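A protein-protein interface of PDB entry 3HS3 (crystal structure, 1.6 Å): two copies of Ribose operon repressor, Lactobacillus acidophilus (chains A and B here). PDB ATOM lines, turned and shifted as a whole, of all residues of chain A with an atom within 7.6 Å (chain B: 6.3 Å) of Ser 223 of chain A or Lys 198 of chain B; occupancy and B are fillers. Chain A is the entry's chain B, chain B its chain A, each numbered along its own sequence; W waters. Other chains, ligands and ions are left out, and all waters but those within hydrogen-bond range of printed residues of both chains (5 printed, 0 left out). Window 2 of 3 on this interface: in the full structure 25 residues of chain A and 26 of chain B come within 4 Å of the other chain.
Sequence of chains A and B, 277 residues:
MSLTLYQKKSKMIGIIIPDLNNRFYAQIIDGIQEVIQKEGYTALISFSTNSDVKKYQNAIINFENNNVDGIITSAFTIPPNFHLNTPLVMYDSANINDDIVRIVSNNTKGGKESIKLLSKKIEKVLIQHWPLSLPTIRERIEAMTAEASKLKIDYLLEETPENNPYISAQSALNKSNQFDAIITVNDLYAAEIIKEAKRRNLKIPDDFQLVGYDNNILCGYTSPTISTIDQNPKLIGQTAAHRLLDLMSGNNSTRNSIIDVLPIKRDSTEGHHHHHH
The side-chain amino group of Lys 195 of chain B lies within hydrogen-bond range of the backbone carbonyl oxygen of Gly 220 of chain A, at 2.8 Å. The side-chain amino group (NZ) of Lys 198 of chain B sits at hydrogen-bond distance from the side-chain hydroxyl (OG) of Ser 223 of chain A.
The backbone carbonyl oxygen of Ser 223 of chain B sits at hydrogen-bond distance from the side-chain amino group of Lys 198 of chain B. The side-chain hydroxyl of Thr 222 of chain B sits at hydrogen-bond distance from the backbone carbonyl oxygen of Pro 224 of chain B, at 2.9 Å. OG1 of Thr 222 of chain A lies within hydrogen-bond range of O of Pro 224 of chain A, at 2.8 Å.
Among the printed residues, pairs that only touch across the chains: Leu 218 of chain A with Tyr 221 of chain B (3.9 Å), Tyr 221 of chain A with Thr 222 of chain B (3.6 Å) and Thr 222 of chain A with Tyr 221 of chain B (3.5 Å).
Ile 204 of chain A touches none of the printed residues of chain B. Of the printed residues of chain B, Leu 218 of chain A touches Tyr 221. Cys 219 of chain A touches none of the printed residues of chain B. Of the printed residues of chain B, Thr 222 of chain A touches Tyr 221 (3.5 Å). Ser 223 of chain A touches one residue of chain B. Lys 198 of chain B touches just one residue of chain A: Ser 223 (2.7 Å). Printed residues of chain A within 4 Å of Tyr 221 of chain B: Leu 218 (3.9 Å) and Thr 222 (3.5 Å). Printed residues of chain A within 4 Å of Thr 222 of chain B: Tyr 221. The nearest residue of chain B that does not touch Ser 223 of chain A is Ser 223 of chain B (4.3 Å).
Of the 17 printed residues of chain A, 5 touch a printed residue of chain B. Hydrophobic or aromatic side chains of chain A that line the printed part of chain B: Leu 218. Along chain B the printed residues that touch a printed residue of chain A span positions 195 to 222. Among the printed residues, no Asp or Glu carboxylate lies within 4 Å of a Lys or Arg side-chain nitrogen of the other chain.
Tyr 221 of chain A touches Thr 222 of chain B, and with the chains exchanged Thr 222 of chain A touches Tyr 221 of chain B. Ser 223 of chain A touches Lys 198 of chain B, but with the chains exchanged Lys 198 of chain A does not touch Ser 223 of chain B (4.4 Å). Positions printed for both chains: 194, 195, 198, 221, 222, 223 and 224. Of the 5 pairs that touch across the chains among the printed residues, 2 have their exchanged pair printed and touching as well.
Water W3 lies within hydrogen-bond range of the backbone carbonyl oxygen of Tyr 221 of chain A, the backbone NH of Ser 223 of chain B, the side-chain hydroxyl of Ser 223 of chain A and the side-chain amino group of Lys 198 of chain B. Water W5 lies within hydrogen-bond range of O of Tyr 221 of chain B (2.7 Å), N of Ser 223 of chain A (2.8 Å) and OG of Ser 223 of chain B (2.9 Å). Water W4 lies within hydrogen-bond range of O of Ser 223 of chain A (2.7 Å) and OG of Ser 223 of chain B (2.9 Å). Water W2 lies within hydrogen-bond range of the side-chain amino group (NZ) of Lys 198 of chain B and the side-chain hydroxyl (OG) of Ser 223 of chain A. Water W1 lies within hydrogen-bond range of the side-chain amino group (NZ) of Lys 198 of chain A and the side-chain hydroxyl (OG) of Ser 223 of chain B.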
ATOM      1  N   ILE A 194      20.839 -11.938  31.153  1.00  0.00           N
ATOM      2  CA  ILE A 194      20.982 -12.351  29.759  1.00  0.00           C
ATOM      3  C   ILE A 194      21.944 -13.537  29.687  1.00  0.00           C
ATOM      4  O   ILE A 194      21.701 -14.501  28.959  1.00  0.00           O
ATOM      5  CB  ILE A 194      21.551 -11.204  28.886  1.00  0.00           C
ATOM      6  CG1 ILE A 194      20.533 -10.068  28.785  1.00  0.00           C
ATOM      7  CG2 ILE A 194      21.910 -11.731  27.493  1.00  0.00           C
ATOM      8  CD1 ILE A 194      21.058  -8.832  28.066  1.00  0.00           C
ATOM      9  N   LYS A 195      23.025 -13.459  30.456  1.00  0.00           N
ATOM     10  CA  LYS A 195      24.039 -14.512  30.476  1.00  0.00           C
ATOM     11  C   LYS A 195      23.492 -15.818  31.052  1.00  0.00           C
ATOM     12  O   LYS A 195      23.780 -16.896  30.536  1.00  0.00           O
ATOM     13  CB  LYS A 195      25.253 -14.048  31.290  1.00  0.00           C
ATOM     14  CG  LYS A 195      26.488 -14.943  31.181  1.00  0.00           C
ATOM     15  CD  LYS A 195      27.605 -14.414  32.069  1.00  0.00           C
ATOM     16  CE  LYS A 195      28.859 -15.273  31.989  1.00  0.00           C
ATOM     17  NZ  LYS A 195      29.501 -15.204  30.654  1.00  0.00           N
ATOM     18  N   LYS A 198      21.075 -17.469  28.666  1.00  0.00           N
ATOM     19  CA  LYS A 198      21.765 -18.186  27.597  1.00  0.00           C
ATOM     20  C   LYS A 198      22.173 -19.566  28.103  1.00  0.00           C
ATOM     21  O   LYS A 198      22.129 -20.548  27.357  1.00  0.00           O
ATOM     22  CB  LYS A 198      23.003 -17.402  27.141  1.00  0.00           C
ATOM     23  CG  LYS A 198      23.654 -17.932  25.864  1.00  0.00           C
ATOM     24  CD  LYS A 198      24.757 -17.003  25.369  1.00  0.00           C
ATOM     25  CE  LYS A 198      25.375 -17.505  24.068  1.00  0.00           C
ATOM     26  NZ  LYS A 198      24.370 -17.597  22.969  1.00  0.00           N
ATOM     27  N   LYS A 203      15.759 -17.197  25.404  1.00  0.00           N
ATOM     28  CA  LYS A 203      16.096 -15.992  24.658  1.00  0.00           C
ATOM     29  C   LYS A 203      15.316 -14.767  25.107  1.00  0.00           C
ATOM     30  O   LYS A 203      14.164 -14.858  25.530  1.00  0.00           O
ATOM     31  CB  LYS A 203      15.872 -16.216  23.158  1.00  0.00           C
ATOM     32  CG  LYS A 203      16.739 -17.313  22.553  1.00  0.00           C
ATOM     33  CD  LYS A 203      16.449 -17.516  21.069  1.00  0.00           C
ATOM     34  CE  LYS A 203      16.922 -16.340  20.220  1.00  0.00           C
ATOM     35  NZ  LYS A 203      18.407 -16.197  20.225  1.00  0.00           N
ATOM     36  N   ILE A 204      15.970 -13.618  25.012  1.00  0.00           N
ATOM     37  CA  ILE A 204      15.376 -12.340  25.375  1.00  0.00           C
ATOM     38  C   ILE A 204      15.405 -11.512  24.097  1.00  0.00           C
ATOM     39  O   ILE A 204      16.432 -11.458  23.415  1.00  0.00           O
ATOM     40  CB  ILE A 204      16.208 -11.649  26.474  1.00  0.00           C
ATOM     41  CG1 ILE A 204      16.231 -12.540  27.719  1.00  0.00           C
ATOM     42  CG2 ILE A 204      15.635 -10.271  26.791  1.00  0.00           C
ATOM     43  CD1 ILE A 204      17.180 -12.079  28.797  1.00  0.00           C
ATOM     44  N   PRO A 205      14.297 -10.834  23.763  1.00  0.00           N
ATOM     45  CA  PRO A 205      13.012 -10.749  24.466  1.00  0.00           C
ATOM     46  C   PRO A 205      12.030 -11.896  24.219  1.00  0.00           C
ATOM     47  O   PRO A 205      10.926 -11.905  24.768  1.00  0.00           O
ATOM     48  CB  PRO A 205      12.456  -9.428  23.966  1.00  0.00           C
ATOM     49  CG  PRO A 205      12.862  -9.458  22.526  1.00  0.00           C
ATOM     50  CD  PRO A 205      14.301  -9.944  22.587  1.00  0.00           C
ATOM     51  N   LEU A 218      27.935  -1.217  28.532  1.00  0.00           N
ATOM     52  CA  LEU A 218      27.653  -2.572  28.071  1.00  0.00           C
ATOM     53  C   LEU A 218      26.289  -2.789  27.423  1.00  0.00           C
ATOM     54  O   LEU A 218      26.100  -3.773  26.710  1.00  0.00           O
ATOM     55  CB  LEU A 218      27.859  -3.575  29.216  1.00  0.00           C
ATOM     56  CG  LEU A 218      27.003  -3.497  30.480  1.00  0.00           C
ATOM     57  CD1 LEU A 218      25.593  -3.981  30.191  1.00  0.00           C
ATOM     58  CD2 LEU A 218      27.634  -4.363  31.558  1.00  0.00           C
ATOM     59  N   CYS A 219      25.344  -1.878  27.647  1.00  0.00           N
ATOM     60  CA  CYS A 219      24.009  -2.034  27.062  1.00  0.00           C
ATOM     61  C   CYS A 219      24.040  -2.179  25.547  1.00  0.00           C
ATOM     62  O   CYS A 219      23.204  -2.865  24.967  1.00  0.00           O
ATOM     63  CB  CYS A 219      23.110  -0.839  27.401  1.00  0.00           C
ATOM     64  SG  CYS A 219      22.634  -0.683  29.129  1.00  0.00           S
ATOM     65  N   GLY A 220      24.996  -1.526  24.900  1.00  0.00           N
ATOM     66  CA  GLY A 220      25.054  -1.605  23.455  1.00  0.00           C
ATOM     67  C   GLY A 220      25.892  -2.738  22.903  1.00  0.00           C
ATOM     68  O   GLY A 220      25.977  -2.895  21.686  1.00  0.00           O
ATOM     69  N   TYR A 221      26.493  -3.534  23.781  1.00  0.00           N
ATOM     70  CA  TYR A 221      27.342  -4.630  23.335  1.00  0.00           C
ATOM     71  C   TYR A 221      26.847  -6.027  23.672  1.00  0.00           C
ATOM     72  O   TYR A 221      27.456  -7.021  23.270  1.00  0.00           O
ATOM     73  CB  TYR A 221      28.750  -4.446  23.893  1.00  0.00           C
ATOM     74  CG  TYR A 221      29.405  -3.166  23.442  1.00  0.00           C
ATOM     75  CD1 TYR A 221      29.753  -2.178  24.360  1.00  0.00           C
ATOM     76  CD2 TYR A 221      29.679  -2.938  22.096  1.00  0.00           C
ATOM     77  CE1 TYR A 221      30.363  -0.994  23.948  1.00  0.00           C
ATOM     78  CE2 TYR A 221      30.287  -1.759  21.673  1.00  0.00           C
ATOM     79  CZ  TYR A 221      30.628  -0.792  22.603  1.00  0.00           C
ATOM     80  OH  TYR A 221      31.238   0.370  22.184  1.00  0.00           O
ATOM     81  N   THR A 222      25.753  -6.110  24.418  1.00  0.00           N
ATOM     82  CA  THR A 222      25.198  -7.407  24.774  1.00  0.00           C
ATOM     83  C   THR A 222      24.230  -7.841  23.687  1.00  0.00           C
ATOM     84  O   THR A 222      23.858  -7.047  22.820  1.00  0.00           O
ATOM     85  CB  THR A 222      24.436  -7.347  26.113  1.00  0.00           C
ATOM     86  OG1 THR A 222      23.477  -6.282  26.074  1.00  0.00           O
ATOM     87  CG2 THR A 222      25.399  -7.110  27.266  1.00  0.00           C
ATOM     88  N   SER A 223      23.836  -9.108  23.728  1.00  0.00           N
ATOM     89  CA  SER A 223      22.882  -9.649  22.767  1.00  0.00           C
ATOM     90  C   SER A 223      21.794 -10.319  23.592  1.00  0.00           C
ATOM     91  O   SER A 223      22.004 -11.396  24.155  1.00  0.00           O
ATOM     92  CB  SER A 223      23.559 -10.666  21.847  1.00  0.00           C
ATOM     93  OG  SER A 223      24.540 -10.034  21.039  1.00  0.00           O
ATOM     94  N   PRO A 224      20.600  -9.710  23.649  1.00  0.00           N
ATOM     95  CA  PRO A 224      20.196  -8.439  23.033  1.00  0.00           C
ATOM     96  C   PRO A 224      20.729  -7.191  23.723  1.00  0.00           C
ATOM     97  O   PRO A 224      21.159  -7.250  24.873  1.00  0.00           O
ATOM     98  CB  PRO A 224      18.678  -8.503  23.124  1.00  0.00           C
ATOM     99  CG  PRO A 224      18.487  -9.141  24.458  1.00  0.00           C
ATOM    100  CD  PRO A 224      19.489 -10.283  24.429  1.00  0.00           C
ATOM    101  N   THR A 225      20.698  -6.064  23.015  1.00  0.00           N
ATOM    102  CA  THR A 225      21.122  -4.798  23.595  1.00  0.00           C
ATOM    103  C   THR A 225      20.075  -4.498  24.669  1.00  0.00           C
ATOM    104  O   THR A 225      18.904  -4.851  24.516  1.00  0.00           O
ATOM    105  CB  THR A 225      21.165  -3.676  22.539  1.00  0.00           C
ATOM    106  OG1 THR A 225      19.949  -3.677  21.785  1.00  0.00           O
ATOM    107  CG2 THR A 225      22.346  -3.894  21.593  1.00  0.00           C
ATOM    108  N   ILE A 226      20.493  -3.837  25.742  1.00  0.00           N
ATOM    109  CA  ILE A 226      19.617  -3.577  26.883  1.00  0.00           C
ATOM    110  C   ILE A 226      18.827  -2.268  26.969  1.00  0.00           C
ATOM    111  O   ILE A 226      19.403  -1.182  26.901  1.00  0.00           O
ATOM    112  CB  ILE A 226      20.443  -3.728  28.176  1.00  0.00           C
ATOM    113  CG1 ILE A 226      21.074  -5.126  28.217  1.00  0.00           C
ATOM    114  CG2 ILE A 226      19.576  -3.479  29.388  1.00  0.00           C
ATOM    115  CD1 ILE A 226      22.087  -5.321  29.321  1.00  0.00           C
ATOM    116  N   ASP A 267      16.980  -3.559  22.035  1.00  0.00           N
ATOM    117  CA  ASP A 267      16.387  -4.833  21.657  1.00  0.00           C
ATOM    118  C   ASP A 267      15.781  -5.713  22.744  1.00  0.00           C
ATOM    119  O   ASP A 267      14.966  -6.586  22.439  1.00  0.00           O
ATOM    120  CB  ASP A 267      17.386  -5.653  20.835  1.00  0.00           C
ATOM    121  CG  ASP A 267      17.733  -4.991  19.509  1.00  0.00           C
ATOM    122  OD1 ASP A 267      16.931  -4.165  19.016  1.00  0.00           O
ATOM    123  OD2 ASP A 267      18.803  -5.305  18.948  1.00  0.00           O
ATOM    124  N   SER A 268      16.140  -5.491  24.005  1.00  0.00           N
ATOM    125  CA  SER A 268      15.601  -6.336  25.065  1.00  0.00           C
ATOM    126  C   SER A 268      14.112  -6.124  25.356  1.00  0.00           C
ATOM    127  O   SER A 268      13.515  -6.902  26.098  1.00  0.00           O
ATOM    128  CB  SER A 268      16.427  -6.189  26.350  1.00  0.00           C
ATOM    129  OG  SER A 268      16.233  -4.931  26.957  1.00  0.00           O
ATOM    130  N   LEU B 173      37.154  -5.085  10.127  1.00  0.00           N
ATOM    131  CA  LEU B 173      36.260  -5.920   9.340  1.00  0.00           C
ATOM    132  C   LEU B 173      36.482  -5.781   7.835  1.00  0.00           C
ATOM    133  O   LEU B 173      36.320  -6.755   7.095  1.00  0.00           O
ATOM    134  CB  LEU B 173      34.794  -5.622   9.685  1.00  0.00           C
ATOM    135  CG  LEU B 173      34.157  -6.451  10.814  1.00  0.00           C
ATOM    136  CD1 LEU B 173      34.183  -7.922  10.428  1.00  0.00           C
ATOM    137  CD2 LEU B 173      34.903  -6.237  12.132  1.00  0.00           C
ATOM    138  N   ILE B 193      34.254  -4.677  17.405  1.00  0.00           N
ATOM    139  CA  ILE B 193      34.536  -5.576  16.295  1.00  0.00           C
ATOM    140  C   ILE B 193      33.463  -6.664  16.247  1.00  0.00           C
ATOM    141  O   ILE B 193      32.996  -7.029  15.176  1.00  0.00           O
ATOM    142  CB  ILE B 193      35.950  -6.197  16.422  1.00  0.00           C
ATOM    143  CG1 ILE B 193      36.993  -5.153  16.011  1.00  0.00           C
ATOM    144  CG2 ILE B 193      36.080  -7.432  15.532  1.00  0.00           C
ATOM    145  CD1 ILE B 193      38.421  -5.606  16.190  1.00  0.00           C
ATOM    146  N   ILE B 194      33.061  -7.165  17.411  1.00  0.00           N
ATOM    147  CA  ILE B 194      32.022  -8.187  17.469  1.00  0.00           C
ATOM    148  C   ILE B 194      30.712  -7.630  16.914  1.00  0.00           C
ATOM    149  O   ILE B 194      30.012  -8.305  16.159  1.00  0.00           O
ATOM    150  CB  ILE B 194      31.789  -8.659  18.921  1.00  0.00           C
ATOM    151  CG1 ILE B 194      32.977  -9.504  19.380  1.00  0.00           C
ATOM    152  CG2 ILE B 194      30.491  -9.464  19.017  1.00  0.00           C
ATOM    153  CD1 ILE B 194      32.916  -9.927  20.838  1.00  0.00           C
ATOM    154  N   LYS B 195      30.395  -6.392  17.280  1.00  0.00           N
ATOM    155  CA  LYS B 195      29.161  -5.762  16.830  1.00  0.00           C
ATOM    156  C   LYS B 195      29.137  -5.565  15.316  1.00  0.00           C
ATOM    157  O   LYS B 195      28.117  -5.814  14.673  1.00  0.00           O
ATOM    158  CB  LYS B 195      28.966  -4.423  17.551  1.00  0.00           C
ATOM    159  CG  LYS B 195      27.537  -3.904  17.521  1.00  0.00           C
ATOM    160  CD  LYS B 195      27.356  -2.747  18.492  1.00  0.00           C
ATOM    161  CE  LYS B 195      25.916  -2.263  18.518  1.00  0.00           C
ATOM    162  NZ  LYS B 195      25.749  -1.161  19.505  1.00  0.00           N
ATOM    163  N   GLU B 196      30.258  -5.133  14.743  1.00  0.00           N
ATOM    164  CA  GLU B 196      30.323  -4.915  13.300  1.00  0.00           C
ATOM    165  C   GLU B 196      30.311  -6.246  12.556  1.00  0.00           C
ATOM    166  O   GLU B 196      29.723  -6.353  11.481  1.00  0.00           O
ATOM    167  CB  GLU B 196      31.576  -4.110  12.942  1.00  0.00           C
ATOM    168  CG  GLU B 196      31.706  -3.739  11.464  1.00  0.00           C
ATOM    169  CD  GLU B 196      30.513  -2.959  10.933  1.00  0.00           C
ATOM    170  OE1 GLU B 196      29.944  -2.139  11.688  1.00  0.00           O
ATOM    171  OE2 GLU B 196      30.156  -3.156   9.751  1.00  0.00           O
ATOM    172  N   ALA B 197      30.955  -7.261  13.125  1.00  0.00           N
ATOM    173  CA  ALA B 197      30.984  -8.572  12.492  1.00  0.00           C
ATOM    174  C   ALA B 197      29.557  -9.083  12.326  1.00  0.00           C
ATOM    175  O   ALA B 197      29.217  -9.668  11.298  1.00  0.00           O
ATOM    176  CB  ALA B 197      31.804  -9.556  13.331  1.00  0.00           C
ATOM    177  N   LYS B 198      28.723  -8.854  13.336  1.00  0.00           N
ATOM    178  CA  LYS B 198      27.334  -9.294  13.283  1.00  0.00           C
ATOM    179  C   LYS B 198      26.557  -8.534  12.220  1.00  0.00           C
ATOM    180  O   LYS B 198      25.662  -9.094  11.584  1.00  0.00           O
ATOM    181  CB  LYS B 198      26.665  -9.128  14.650  1.00  0.00           C
ATOM    182  CG  LYS B 198      27.140 -10.147  15.673  1.00  0.00           C
ATOM    183  CD  LYS B 198      26.527  -9.903  17.043  1.00  0.00           C
ATOM    184  CE  LYS B 198      27.113 -10.856  18.081  1.00  0.00           C
ATOM    185  NZ  LYS B 198      26.699 -10.513  19.473  1.00  0.00           N
ATOM    186  N   ARG B 199      26.900  -7.266  12.014  1.00  0.00           N
ATOM    187  CA  ARG B 199      26.219  -6.467  10.995  1.00  0.00           C
ATOM    188  C   ARG B 199      26.531  -7.028   9.615  1.00  0.00           C
ATOM    189  O   ARG B 199      25.726  -6.917   8.691  1.00  0.00           O
ATOM    190  CB  ARG B 199      26.673  -5.004  11.039  1.00  0.00           C
ATOM    191  CG  ARG B 199      26.364  -4.266  12.329  1.00  0.00           C
ATOM    192  CD  ARG B 199      26.443  -2.755  12.120  1.00  0.00           C
ATOM    193  NE  ARG B 199      26.228  -2.031  13.369  1.00  0.00           N
ATOM    194  CZ  ARG B 199      27.189  -1.708  14.227  1.00  0.00           C
ATOM    195  NH1 ARG B 199      28.451  -2.034  13.972  1.00  0.00           N
ATOM    196  NH2 ARG B 199      26.887  -1.073  15.350  1.00  0.00           N
ATOM    197  N   ARG B 200      27.706  -7.634   9.484  1.00  0.00           N
ATOM    198  CA  ARG B 200      28.140  -8.193   8.211  1.00  0.00           C
ATOM    199  C   ARG B 200      27.913  -9.696   8.115  1.00  0.00           C
ATOM    200  O   ARG B 200      28.390 -10.351   7.186  1.00  0.00           O
ATOM    201  CB  ARG B 200      29.616  -7.865   7.985  1.00  0.00           C
ATOM    202  CG  ARG B 200      29.925  -6.381   8.151  1.00  0.00           C
ATOM    203  CD  ARG B 200      31.320  -6.037   7.664  1.00  0.00           C
ATOM    204  NE  ARG B 200      31.648  -4.639   7.921  1.00  0.00           N
ATOM    205  CZ  ARG B 200      32.674  -3.999   7.373  1.00  0.00           C
ATOM    206  NH1 ARG B 200      33.477  -4.633   6.528  1.00  0.00           N
ATOM    207  NH2 ARG B 200      32.905  -2.728   7.676  1.00  0.00           N
ATOM    208  N   ASN B 201      27.176 -10.236   9.079  1.00  0.00           N
ATOM    209  CA  ASN B 201      26.867 -11.657   9.112  1.00  0.00           C
ATOM    210  C   ASN B 201      28.108 -12.543   9.137  1.00  0.00           C
ATOM    211  O   ASN B 201      28.164 -13.574   8.462  1.00  0.00           O
ATOM    212  CB  ASN B 201      25.989 -12.035   7.915  1.00  0.00           C
ATOM    213  CG  ASN B 201      24.654 -11.314   7.920  1.00  0.00           C
ATOM    214  OD1 ASN B 201      23.922 -11.346   8.910  1.00  0.00           O
ATOM    215  ND2 ASN B 201      24.329 -10.663   6.808  1.00  0.00           N
ATOM    216  N   LEU B 202      29.107 -12.123   9.906  1.00  0.00           N
ATOM    217  CA  LEU B 202      30.336 -12.888  10.063  1.00  0.00           C
ATOM    218  C   LEU B 202      30.330 -13.415  11.495  1.00  0.00           C
ATOM    219  O   LEU B 202      29.749 -12.792  12.384  1.00  0.00           O
ATOM    220  CB  LEU B 202      31.562 -12.002   9.822  1.00  0.00           C
ATOM    221  CG  LEU B 202      31.789 -11.599   8.361  1.00  0.00           C
ATOM    222  CD1 LEU B 202      32.902 -10.564   8.249  1.00  0.00           C
ATOM    223  CD2 LEU B 202      32.136 -12.851   7.563  1.00  0.00           C
ATOM    224  N   TYR B 221      30.127 -10.463  29.143  1.00  0.00           N
ATOM    225  CA  TYR B 221      28.751 -10.154  28.778  1.00  0.00           C
ATOM    226  C   TYR B 221      28.473 -10.084  27.281  1.00  0.00           C
ATOM    227  O   TYR B 221      27.317  -9.969  26.868  1.00  0.00           O
ATOM    228  CB  TYR B 221      28.341  -8.846  29.451  1.00  0.00           C
ATOM    229  CG  TYR B 221      28.347  -8.941  30.958  1.00  0.00           C
ATOM    230  CD1 TYR B 221      29.048  -8.022  31.734  1.00  0.00           C
ATOM    231  CD2 TYR B 221      27.645  -9.950  31.609  1.00  0.00           C
ATOM    232  CE1 TYR B 221      29.046  -8.109  33.127  1.00  0.00           C
ATOM    233  CE2 TYR B 221      27.636 -10.045  32.997  1.00  0.00           C
ATOM    234  CZ  TYR B 221      28.336  -9.121  33.749  1.00  0.00           C
ATOM    235  OH  TYR B 221      28.305  -9.208  35.124  1.00  0.00           O
ATOM    236  N   THR B 222      29.522 -10.150  26.469  1.00  0.00           N
ATOM    237  CA  THR B 222      29.349 -10.116  25.021  1.00  0.00           C
ATOM    238  C   THR B 222      29.161 -11.528  24.471  1.00  0.00           C
ATOM    239  O   THR B 222      29.328 -12.513  25.186  1.00  0.00           O
ATOM    240  CB  THR B 222      30.563  -9.462  24.309  1.00  0.00           C
ATOM    241  OG1 THR B 222      31.777 -10.124  24.696  1.00  0.00           O
ATOM    242  CG2 THR B 222      30.660  -7.983  24.668  1.00  0.00           C
ATOM    243  N   SER B 223      28.791 -11.620  23.199  1.00  0.00           N
ATOM    244  CA  SER B 223      28.600 -12.917  22.556  1.00  0.00           C
ATOM    245  C   SER B 223      29.239 -12.852  21.182  1.00  0.00           C
ATOM    246  O   SER B 223      28.717 -12.200  20.277  1.00  0.00           O
ATOM    247  CB  SER B 223      27.110 -13.239  22.422  1.00  0.00           C
ATOM    248  OG  SER B 223      26.491 -13.283  23.697  1.00  0.00           O
ATOM    249  N   PRO B 224      30.378 -13.538  20.999  1.00  0.00           N
ATOM    250  CA  PRO B 224      31.106 -14.360  21.972  1.00  0.00           C
ATOM    251  C   PRO B 224      31.777 -13.568  23.087  1.00  0.00           C
ATOM    252  O   PRO B 224      32.042 -12.369  22.944  1.00  0.00           O
ATOM    253  CB  PRO B 224      32.142 -15.063  21.105  1.00  0.00           C
ATOM    254  CG  PRO B 224      32.489 -13.989  20.114  1.00  0.00           C
ATOM    255  CD  PRO B 224      31.116 -13.475  19.725  1.00  0.00           C
HETATM  256  O   HOH W   1      23.856 -14.630  21.953  1.00  0.00           O
HETATM  257  O   HOH W   2      24.542 -12.762  19.026  1.00  0.00           O
HETATM  258  O   HOH W   3      27.198  -9.455  22.181  1.00  0.00           O
HETATM  259  O   HOH W   4      23.806 -13.407  24.659  1.00  0.00           O
HETATM  260  O   HOH W   5      25.580 -10.867  25.013  1.00  0.00           O
